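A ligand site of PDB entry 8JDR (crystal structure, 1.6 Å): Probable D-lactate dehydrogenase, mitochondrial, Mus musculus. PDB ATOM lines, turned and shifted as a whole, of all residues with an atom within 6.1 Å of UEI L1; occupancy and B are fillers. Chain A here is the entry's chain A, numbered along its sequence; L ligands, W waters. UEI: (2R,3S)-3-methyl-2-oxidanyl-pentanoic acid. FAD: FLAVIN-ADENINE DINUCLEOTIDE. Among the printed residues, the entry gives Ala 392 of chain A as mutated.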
ATOM      1  N   THR A  86     -19.208   0.549 -14.712  1.00  0.00           N
ATOM      2  CA  THR A  86     -20.569   0.085 -14.936  1.00  0.00           C
ATOM      3  C   THR A  86     -20.641  -1.410 -15.233  1.00  0.00           C
ATOM      4  O   THR A  86     -21.734  -1.918 -15.495  1.00  0.00           O
ATOM      5  CB  THR A  86     -21.256   0.864 -16.061  1.00  0.00           C
ATOM      6  OG1 THR A  86     -20.676   0.527 -17.338  1.00  0.00           O
ATOM      7  CG2 THR A  86     -21.140   2.357 -15.833  1.00  0.00           C
ATOM      8  N   VAL A  88     -20.804  -5.527 -14.663  1.00  0.00           N
ATOM      9  CA  VAL A  88     -21.705  -6.268 -13.772  1.00  0.00           C
ATOM     10  C   VAL A  88     -21.134  -7.614 -13.367  1.00  0.00           C
ATOM     11  O   VAL A  88     -21.867  -8.480 -12.883  1.00  0.00           O
ATOM     12  CB  VAL A  88     -23.097  -6.419 -14.398  1.00  0.00           C
ATOM     13  CG1 VAL A  88     -23.755  -5.054 -14.554  1.00  0.00           C
ATOM     14  CG2 VAL A  88     -23.050  -7.130 -15.746  1.00  0.00           C
ATOM     15  N   GLY A 146     -26.951   0.040 -22.061  1.00  0.00           N
ATOM     16  CA  GLY A 146     -27.806   1.017 -21.421  1.00  0.00           C
ATOM     17  C   GLY A 146     -27.068   2.008 -20.542  1.00  0.00           C
ATOM     18  O   GLY A 146     -27.591   3.107 -20.290  1.00  0.00           O
ATOM     19  N   GLU A 264     -36.062  -6.481 -28.766  1.00  0.00           N
ATOM     20  CA  GLU A 264     -35.777  -6.656 -27.348  1.00  0.00           C
ATOM     21  C   GLU A 264     -36.989  -7.280 -26.662  1.00  0.00           C
ATOM     22  O   GLU A 264     -38.131  -6.892 -26.940  1.00  0.00           O
ATOM     23  CB  GLU A 264     -35.460  -5.336 -26.700  1.00  0.00           C
ATOM     24  CG  GLU A 264     -34.149  -4.728 -27.176  1.00  0.00           C
ATOM     25  CD  GLU A 264     -32.959  -5.448 -26.634  1.00  0.00           C
ATOM     26  OE1 GLU A 264     -32.956  -5.752 -25.425  1.00  0.00           O
ATOM     27  OE2 GLU A 264     -32.010  -5.716 -27.400  1.00  0.00           O
ATOM     28  N   ARG A 334     -35.953   1.117 -21.879  1.00  0.00           N
ATOM     29  CA  ARG A 334     -35.266  -0.155 -22.046  1.00  0.00           C
ATOM     30  C   ARG A 334     -33.836  -0.076 -21.526  1.00  0.00           C
ATOM     31  O   ARG A 334     -33.377  -0.960 -20.804  1.00  0.00           O
ATOM     32  CB  ARG A 334     -35.281  -0.580 -23.508  1.00  0.00           C
ATOM     33  CG  ARG A 334     -34.298  -1.719 -23.842  1.00  0.00           C
ATOM     34  CD  ARG A 334     -34.693  -3.040 -23.176  1.00  0.00           C
ATOM     35  NE  ARG A 334     -33.668  -4.050 -23.413  1.00  0.00           N
ATOM     36  CZ  ARG A 334     -32.596  -4.226 -22.628  1.00  0.00           C
ATOM     37  NH1 ARG A 334     -32.399  -3.474 -21.542  1.00  0.00           N
ATOM     38  NH2 ARG A 334     -31.708  -5.158 -22.954  1.00  0.00           N
ATOM     39  N   HIS A 335     -33.126   0.994 -21.881  1.00  0.00           N
ATOM     40  CA  HIS A 335     -31.743   1.127 -21.431  1.00  0.00           C
ATOM     41  C   HIS A 335     -31.640   1.197 -19.922  1.00  0.00           C
ATOM     42  O   HIS A 335     -30.586   0.858 -19.353  1.00  0.00           O
ATOM     43  CB  HIS A 335     -31.125   2.385 -22.053  1.00  0.00           C
ATOM     44  CG  HIS A 335     -30.694   2.209 -23.487  1.00  0.00           C
ATOM     45  ND1 HIS A 335     -30.745   3.241 -24.406  1.00  0.00           N
ATOM     46  CD2 HIS A 335     -30.189   1.139 -24.148  1.00  0.00           C
ATOM     47  CE1 HIS A 335     -30.286   2.805 -25.575  1.00  0.00           C
ATOM     48  NE2 HIS A 335     -29.940   1.535 -25.437  1.00  0.00           N
ATOM     49  N   ASN A 336     -32.694   1.626 -19.241  1.00  0.00           N
ATOM     50  CA  ASN A 336     -32.643   1.750 -17.793  1.00  0.00           C
ATOM     51  C   ASN A 336     -33.308   0.558 -17.092  1.00  0.00           C
ATOM     52  O   ASN A 336     -33.559   0.626 -15.876  1.00  0.00           O
ATOM     53  CB  ASN A 336     -33.278   3.075 -17.396  1.00  0.00           C
ATOM     54  CG  ASN A 336     -32.270   4.209 -17.429  1.00  0.00           C
ATOM     55  OD1 ASN A 336     -31.446   4.364 -16.533  1.00  0.00           O
ATOM     56  ND2 ASN A 336     -32.313   4.990 -18.502  1.00  0.00           N
ATOM     57  N   ALA A 337     -33.546  -0.541 -17.822  1.00  0.00           N
ATOM     58  CA  ALA A 337     -34.207  -1.717 -17.237  1.00  0.00           C
ATOM     59  C   ALA A 337     -33.501  -2.231 -15.992  1.00  0.00           C
ATOM     60  O   ALA A 337     -34.150  -2.684 -15.037  1.00  0.00           O
ATOM     61  CB  ALA A 337     -34.291  -2.834 -18.283  1.00  0.00           C
ATOM     62  N   TRP A 338     -32.173  -2.213 -15.984  1.00  0.00           N
ATOM     63  CA  TRP A 338     -31.422  -2.634 -14.809  1.00  0.00           C
ATOM     64  C   TRP A 338     -31.857  -1.857 -13.575  1.00  0.00           C
ATOM     65  O   TRP A 338     -32.133  -2.433 -12.518  1.00  0.00           O
ATOM     66  CB  TRP A 338     -29.926  -2.460 -15.067  1.00  0.00           C
ATOM     67  CG  TRP A 338     -29.011  -2.674 -13.900  1.00  0.00           C
ATOM     68  CD1 TRP A 338     -28.361  -1.717 -13.181  1.00  0.00           C
ATOM     69  CD2 TRP A 338     -28.609  -3.934 -13.349  1.00  0.00           C
ATOM     70  NE1 TRP A 338     -27.570  -2.301 -12.213  1.00  0.00           N
ATOM     71  CE2 TRP A 338     -27.710  -3.655 -12.292  1.00  0.00           C
ATOM     72  CE3 TRP A 338     -28.914  -5.257 -13.642  1.00  0.00           C
ATOM     73  CZ2 TRP A 338     -27.136  -4.659 -11.532  1.00  0.00           C
ATOM     74  CZ3 TRP A 338     -28.339  -6.262 -12.882  1.00  0.00           C
ATOM     75  CH2 TRP A 338     -27.466  -5.951 -11.844  1.00  0.00           C
ATOM     76  N   SER A 352     -27.043 -10.504 -12.545  1.00  0.00           N
ATOM     77  CA  SER A 352     -27.664 -10.680 -13.856  1.00  0.00           C
ATOM     78  C   SER A 352     -27.002 -11.849 -14.552  1.00  0.00           C
ATOM     79  O   SER A 352     -25.766 -11.944 -14.591  1.00  0.00           O
ATOM     80  CB  SER A 352     -27.558  -9.410 -14.711  1.00  0.00           C
ATOM     81  OG  SER A 352     -27.978  -9.670 -16.058  1.00  0.00           O
ATOM     82  N   THR A 353     -27.814 -12.745 -15.094  1.00  0.00           N
ATOM     83  CA  THR A 353     -27.319 -13.742 -16.028  1.00  0.00           C
ATOM     84  C   THR A 353     -27.260 -13.141 -17.421  1.00  0.00           C
ATOM     85  O   THR A 353     -27.707 -12.010 -17.664  1.00  0.00           O
ATOM     86  CB  THR A 353     -28.204 -14.984 -16.023  1.00  0.00           C
ATOM     87  OG1 THR A 353     -29.505 -14.653 -16.522  1.00  0.00           O
ATOM     88  CG2 THR A 353     -28.322 -15.585 -14.617  1.00  0.00           C
ATOM     89  N   ASP A 354     -26.673 -13.895 -18.363  1.00  0.00           N
ATOM     90  CA  ASP A 354     -26.373 -13.325 -19.662  1.00  0.00           C
ATOM     91  C   ASP A 354     -26.142 -14.398 -20.722  1.00  0.00           C
ATOM     92  O   ASP A 354     -25.332 -14.221 -21.635  1.00  0.00           O
ATOM     93  CB  ASP A 354     -25.129 -12.416 -19.538  1.00  0.00           C
ATOM     94  CG  ASP A 354     -24.804 -11.674 -20.826  1.00  0.00           C
ATOM     95  OD1 ASP A 354     -25.743 -11.263 -21.549  1.00  0.00           O
ATOM     96  OD2 ASP A 354     -23.585 -11.504 -21.101  1.00  0.00           O
ATOM     97  N   VAL A 383     -35.142  -9.773 -19.418  1.00  0.00           N
ATOM     98  CA  VAL A 383     -35.017  -8.757 -20.467  1.00  0.00           C
ATOM     99  C   VAL A 383     -33.900  -9.217 -21.387  1.00  0.00           C
ATOM    100  O   VAL A 383     -32.961  -9.870 -20.939  1.00  0.00           O
ATOM    101  CB  VAL A 383     -34.717  -7.363 -19.864  1.00  0.00           C
ATOM    102  CG1 VAL A 383     -33.301  -7.316 -19.243  1.00  0.00           C
ATOM    103  CG2 VAL A 383     -34.882  -6.261 -20.893  1.00  0.00           C
ATOM    104  N   GLY A 384     -33.984  -8.911 -22.665  1.00  0.00           N
ATOM    105  CA  GLY A 384     -32.866  -9.433 -23.446  1.00  0.00           C
ATOM    106  C   GLY A 384     -32.777  -9.032 -24.896  1.00  0.00           C
ATOM    107  O   GLY A 384     -33.781  -8.812 -25.581  1.00  0.00           O
ATOM    108  N   HIS A 385     -31.531  -9.042 -25.372  1.00  0.00           N
ATOM    109  CA  HIS A 385     -31.161  -8.942 -26.767  1.00  0.00           C
ATOM    110  C   HIS A 385     -31.470 -10.250 -27.481  1.00  0.00           C
ATOM    111  O   HIS A 385     -30.541 -10.956 -27.924  1.00  0.00           O
ATOM    112  CB  HIS A 385     -29.672  -8.623 -26.900  1.00  0.00           C
ATOM    113  CG  HIS A 385     -29.197  -7.492 -26.029  1.00  0.00           C
ATOM    114  ND1 HIS A 385     -29.755  -6.234 -26.076  1.00  0.00           N
ATOM    115  CD2 HIS A 385     -28.200  -7.434 -25.113  1.00  0.00           C
ATOM    116  CE1 HIS A 385     -29.126  -5.448 -25.215  1.00  0.00           C
ATOM    117  NE2 HIS A 385     -28.166  -6.148 -24.632  1.00  0.00           N
ATOM    118  N   ALA A 392     -31.069 -11.730 -20.344  1.00  0.00           N
ATOM    119  CA  ALA A 392     -30.629 -11.576 -18.958  1.00  0.00           C
ATOM    120  C   ALA A 392     -31.788 -11.860 -18.017  1.00  0.00           C
ATOM    121  O   ALA A 392     -32.925 -11.465 -18.259  1.00  0.00           O
ATOM    122  CB  ALA A 392     -30.102 -10.152 -18.695  1.00  0.00           C
ATOM    123  N   ILE A 394     -32.485 -10.752 -14.269  1.00  0.00           N
ATOM    124  CA  ILE A 394     -32.064  -9.802 -13.250  1.00  0.00           C
ATOM    125  C   ILE A 394     -32.638 -10.293 -11.922  1.00  0.00           C
ATOM    126  O   ILE A 394     -33.861 -10.306 -11.755  1.00  0.00           O
ATOM    127  CB  ILE A 394     -32.541  -8.378 -13.555  1.00  0.00           C
ATOM    128  CG1 ILE A 394     -32.029  -7.935 -14.935  1.00  0.00           C
ATOM    129  CG2 ILE A 394     -32.078  -7.426 -12.443  1.00  0.00           C
ATOM    130  CD1 ILE A 394     -32.499  -6.562 -15.344  1.00  0.00           C
ATOM    131  N   GLU A 429     -22.371 -11.004 -23.599  1.00  0.00           N
ATOM    132  CA  GLU A 429     -21.792  -9.656 -23.665  1.00  0.00           C
ATOM    133  C   GLU A 429     -21.170  -9.137 -22.372  1.00  0.00           C
ATOM    134  O   GLU A 429     -20.233  -8.328 -22.442  1.00  0.00           O
ATOM    135  CB  GLU A 429     -22.851  -8.637 -24.122  1.00  0.00           C
ATOM    136  CG  GLU A 429     -24.164  -8.675 -23.294  1.00  0.00           C
ATOM    137  CD  GLU A 429     -25.126  -7.551 -23.619  1.00  0.00           C
ATOM    138  OE1 GLU A 429     -25.031  -6.969 -24.723  1.00  0.00           O
ATOM    139  OE2 GLU A 429     -26.051  -7.285 -22.793  1.00  0.00           O
ATOM    140  N   HIS A 430     -21.663  -9.543 -21.197  1.00  0.00           N
ATOM    141  CA  HIS A 430     -21.190  -8.911 -19.971  1.00  0.00           C
ATOM    142  C   HIS A 430     -19.770  -9.321 -19.613  1.00  0.00           C
ATOM    143  O   HIS A 430     -19.044  -8.548 -18.974  1.00  0.00           O
ATOM    144  CB  HIS A 430     -22.083  -9.286 -18.796  1.00  0.00           C
ATOM    145  CG  HIS A 430     -23.461  -8.756 -18.905  1.00  0.00           C
ATOM    146  ND1 HIS A 430     -24.514  -9.331 -18.241  1.00  0.00           N
ATOM    147  CD2 HIS A 430     -23.955  -7.700 -19.581  1.00  0.00           C
ATOM    148  CE1 HIS A 430     -25.621  -8.658 -18.509  1.00  0.00           C
ATOM    149  NE2 HIS A 430     -25.308  -7.660 -19.333  1.00  0.00           N
HETATM  150  CAA UEI L   1     -29.212  -4.595 -20.420  1.00  0.00           C
HETATM  151  CAB UEI L   1     -28.144  -4.965 -19.398  1.00  0.00           C
HETATM  152  CAC UEI L   1     -28.810  -5.471 -18.131  1.00  0.00           C
HETATM  153  CAD UEI L   1     -27.737  -5.948 -17.147  1.00  0.00           C
HETATM  154  CAE UEI L   1     -26.924  -4.737 -16.701  1.00  0.00           C
HETATM  155  CAI UEI L   1     -29.739  -6.636 -18.443  1.00  0.00           C
HETATM  156  OAF UEI L   1     -27.356  -5.950 -20.016  1.00  0.00           O
HETATM  157  OAG UEI L   1     -29.944  -3.584 -20.250  1.00  0.00           O
HETATM  158  OAH UEI L   1     -29.347  -5.343 -21.425  1.00  0.00           O
HETATM  159  PA  FAD L   2     -15.644  -1.151 -15.873  1.00  0.00           P
HETATM  160  O1A FAD L   2     -14.918   0.088 -15.549  1.00  0.00           O
HETATM  161  O2A FAD L   2     -16.669  -1.658 -14.891  1.00  0.00           O
HETATM  162  O5B FAD L   2     -14.617  -2.305 -16.226  1.00  0.00           O
HETATM  163  C5B FAD L   2     -15.085  -3.577 -16.723  1.00  0.00           C
HETATM  164  C4B FAD L   2     -13.927  -4.521 -16.930  1.00  0.00           C
HETATM  165  O4B FAD L   2     -13.120  -4.085 -18.048  1.00  0.00           O
HETATM  166  C3B FAD L   2     -12.970  -4.634 -15.743  1.00  0.00           C
HETATM  167  O3B FAD L   2     -12.417  -5.943 -15.702  1.00  0.00           O
HETATM  168  C2B FAD L   2     -11.908  -3.579 -16.071  1.00  0.00           C
HETATM  169  O2B FAD L   2     -10.638  -3.902 -15.498  1.00  0.00           O
HETATM  170  C1B FAD L   2     -11.846  -3.656 -17.589  1.00  0.00           C
HETATM  171  N9A FAD L   2     -11.532  -2.410 -18.254  1.00  0.00           N
HETATM  172  C8A FAD L   2     -12.236  -1.229 -18.256  1.00  0.00           C
HETATM  173  N7A FAD L   2     -11.708  -0.294 -19.006  1.00  0.00           N
HETATM  174  C5A FAD L   2     -10.584  -0.895 -19.552  1.00  0.00           C
HETATM  175  C6A FAD L   2      -9.592  -0.446 -20.439  1.00  0.00           C
HETATM  176  N6A FAD L   2      -9.560   0.790 -20.961  1.00  0.00           N
HETATM  177  N1A FAD L   2      -8.602  -1.299 -20.756  1.00  0.00           N
HETATM  178  C2A FAD L   2      -8.613  -2.531 -20.246  1.00  0.00           C
HETATM  179  N3A FAD L   2      -9.514  -3.076 -19.408  1.00  0.00           N
HETATM  180  C4A FAD L   2     -10.467  -2.204 -19.097  1.00  0.00           C
HETATM  181  N1  FAD L   2     -23.115  -4.387 -21.172  1.00  0.00           N
HETATM  182  C2  FAD L   2     -23.368  -4.885 -22.422  1.00  0.00           C
HETATM  183  O2  FAD L   2     -22.522  -5.550 -23.045  1.00  0.00           O
HETATM  184  N3  FAD L   2     -24.594  -4.630 -23.029  1.00  0.00           N
HETATM  185  C4  FAD L   2     -25.627  -3.902 -22.486  1.00  0.00           C
HETATM  186  O4  FAD L   2     -26.679  -3.762 -23.127  1.00  0.00           O
HETATM  187  C4X FAD L   2     -25.357  -3.360 -21.175  1.00  0.00           C
HETATM  188  N5  FAD L   2     -26.296  -2.627 -20.580  1.00  0.00           N
HETATM  189  C5X FAD L   2     -26.026  -2.135 -19.320  1.00  0.00           C
HETATM  190  C6  FAD L   2     -26.996  -1.350 -18.681  1.00  0.00           C
HETATM  191  C7  FAD L   2     -26.775  -0.831 -17.407  1.00  0.00           C
HETATM  192  C7M FAD L   2     -27.848  -0.009 -16.739  1.00  0.00           C
HETATM  193  C8  FAD L   2     -25.561  -1.096 -16.747  1.00  0.00           C
HETATM  194  C8M FAD L   2     -25.296  -0.534 -15.374  1.00  0.00           C
HETATM  195  C9  FAD L   2     -24.580  -1.853 -17.385  1.00  0.00           C
HETATM  196  C9A FAD L   2     -24.805  -2.381 -18.660  1.00  0.00           C
HETATM  197  N10 FAD L   2     -23.829  -3.145 -19.334  1.00  0.00           N
HETATM  198  C10 FAD L   2     -24.073  -3.657 -20.587  1.00  0.00           C
HETATM  199  C1' FAD L   2     -22.555  -3.507 -18.672  1.00  0.00           C
HETATM  200  C2' FAD L   2     -21.446  -2.480 -18.817  1.00  0.00           C
HETATM  201  O2' FAD L   2     -22.006  -1.209 -19.088  1.00  0.00           O
HETATM  202  C3' FAD L   2     -20.502  -2.918 -19.942  1.00  0.00           C
HETATM  203  O3' FAD L   2     -19.922  -4.170 -19.570  1.00  0.00           O
HETATM  204  C4' FAD L   2     -19.411  -1.888 -20.214  1.00  0.00           C
HETATM  205  O4' FAD L   2     -18.645  -2.324 -21.336  1.00  0.00           O
HETATM  206  C5' FAD L   2     -18.517  -1.669 -19.011  1.00  0.00           C
HETATM  207  O5' FAD L   2     -17.631  -0.562 -19.283  1.00  0.00           O
HETATM  208  P   FAD L   2     -16.955   0.221 -18.105  1.00  0.00           P
HETATM  209  O1P FAD L   2     -18.030   0.894 -17.253  1.00  0.00           O
HETATM  210  O2P FAD L   2     -15.860   1.132 -18.577  1.00  0.00           O
HETATM  211  O3P FAD L   2     -16.359  -1.009 -17.286  1.00  0.00           O
HETATM  212  O   HOH W   1     -29.637  -1.638 -22.117  1.00  0.00           O
HETATM  213  O   HOH W   2     -27.525  -9.075 -21.472  1.00  0.00           O
HETATM  214  O   HOH W   3     -30.561  -1.827 -18.332  1.00  0.00           O
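The side-chain carboxylate (OE2) of Glu 429 is in hydrogen-bond range of an oxygen (OAF) of UEI L1.
N of Thr 86 sits at hydrogen-bond distance from O1P of FAD L2 (2.8 Å).
The side-chain carboxylate of Glu 429 sits at hydrogen-bond distance from a nitrogen (N3) of FAD L2.
The side-chain hydroxyl of Thr 86 is in hydrogen-bond range of an oxygen (O1P) of FAD L2, 2.7 Å away.
NH1 of Arg 334 lies within salt-bridge range of OAG of UEI L1 (2.8 Å).
The backbone NH (N) of Gly 146 is in hydrogen-bond range of a nitrogen (N5) of FAD L2, 3.1 Å away.
A ring nitrogen (NE2) of His 385 is in hydrogen-bond range of an oxygen (O4) of FAD L2, 3.2 Å away.
NE2 of His 430 sits at hydrogen-bond distance from OAF of UEI L1, at 2.8 Å.
The backbone NH (N) of Glu 429 is in hydrogen-bond range of the side-chain carboxylate (OD2) of Asp 354 (2.8 Å).
The guanidinium group (NE) of Arg 334 lies within salt-bridge range of the side-chain carboxylate (OE1) of Glu 264, at 2.7 Å.
A ring nitrogen (ND1) of His 385 sits at hydrogen-bond distance from the side-chain carboxylate (OE2) of Glu 264 (2.7 Å).
The backbone carbonyl oxygen of Val 383 is in hydrogen-bond range of the backbone NH of Ala 392.
The backbone NH (N) of His 430 lies within hydrogen-bond range of the side-chain carboxylate (OD2) of Asp 354 (2.7 Å).
NE2 of His 385 is in hydrogen-bond range of OE2 of Glu 429 (3.0 Å).
CG1 of Val 88 touches CAE of UEI L1, 3.8 Å away.
Trp 338 touches UEI L1.
OG of Ser 352 touches CAD of UEI L1, 3.9 Å away.
Val 383 touches UEI L1.
NE2 of His 385 touches OAH of UEI L1, 3.5 Å away.
Ala 392 touches UEI L1 (CB to CAI, 3.5 Å).
Hydrophobic or aromatic side chains that line UEI L1: Val 88, Trp 338, Val 383, His 385, Ala 392 and His 430.
Within 4 Å of UEI L1: Val 88, Arg 334, Trp 338, Ser 352, Val 383, His 385, Ala 392, Glu 429 and His 430.
Water W3 lies within hydrogen-bond range of an oxygen (OAG) of UEI L1 (2.7 Å), the backbone carbonyl oxygen (O) of His 335 (2.9 Å), the backbone NH (N) of Trp 338 (2.9 Å) and the backbone NH (N) of Ala 337 (3.3 Å).
Water W1 lies within hydrogen-bond range of OAG of UEI L1 (2.7 Å), N of Gly 146 (3.2 Å) and NH1 of Arg 334 (3.4 Å).
Water W2 lies within hydrogen-bond range of OE2 of Glu 429, OD1 of Asp 354, NE2 of His 430 and OAF of UEI L1.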
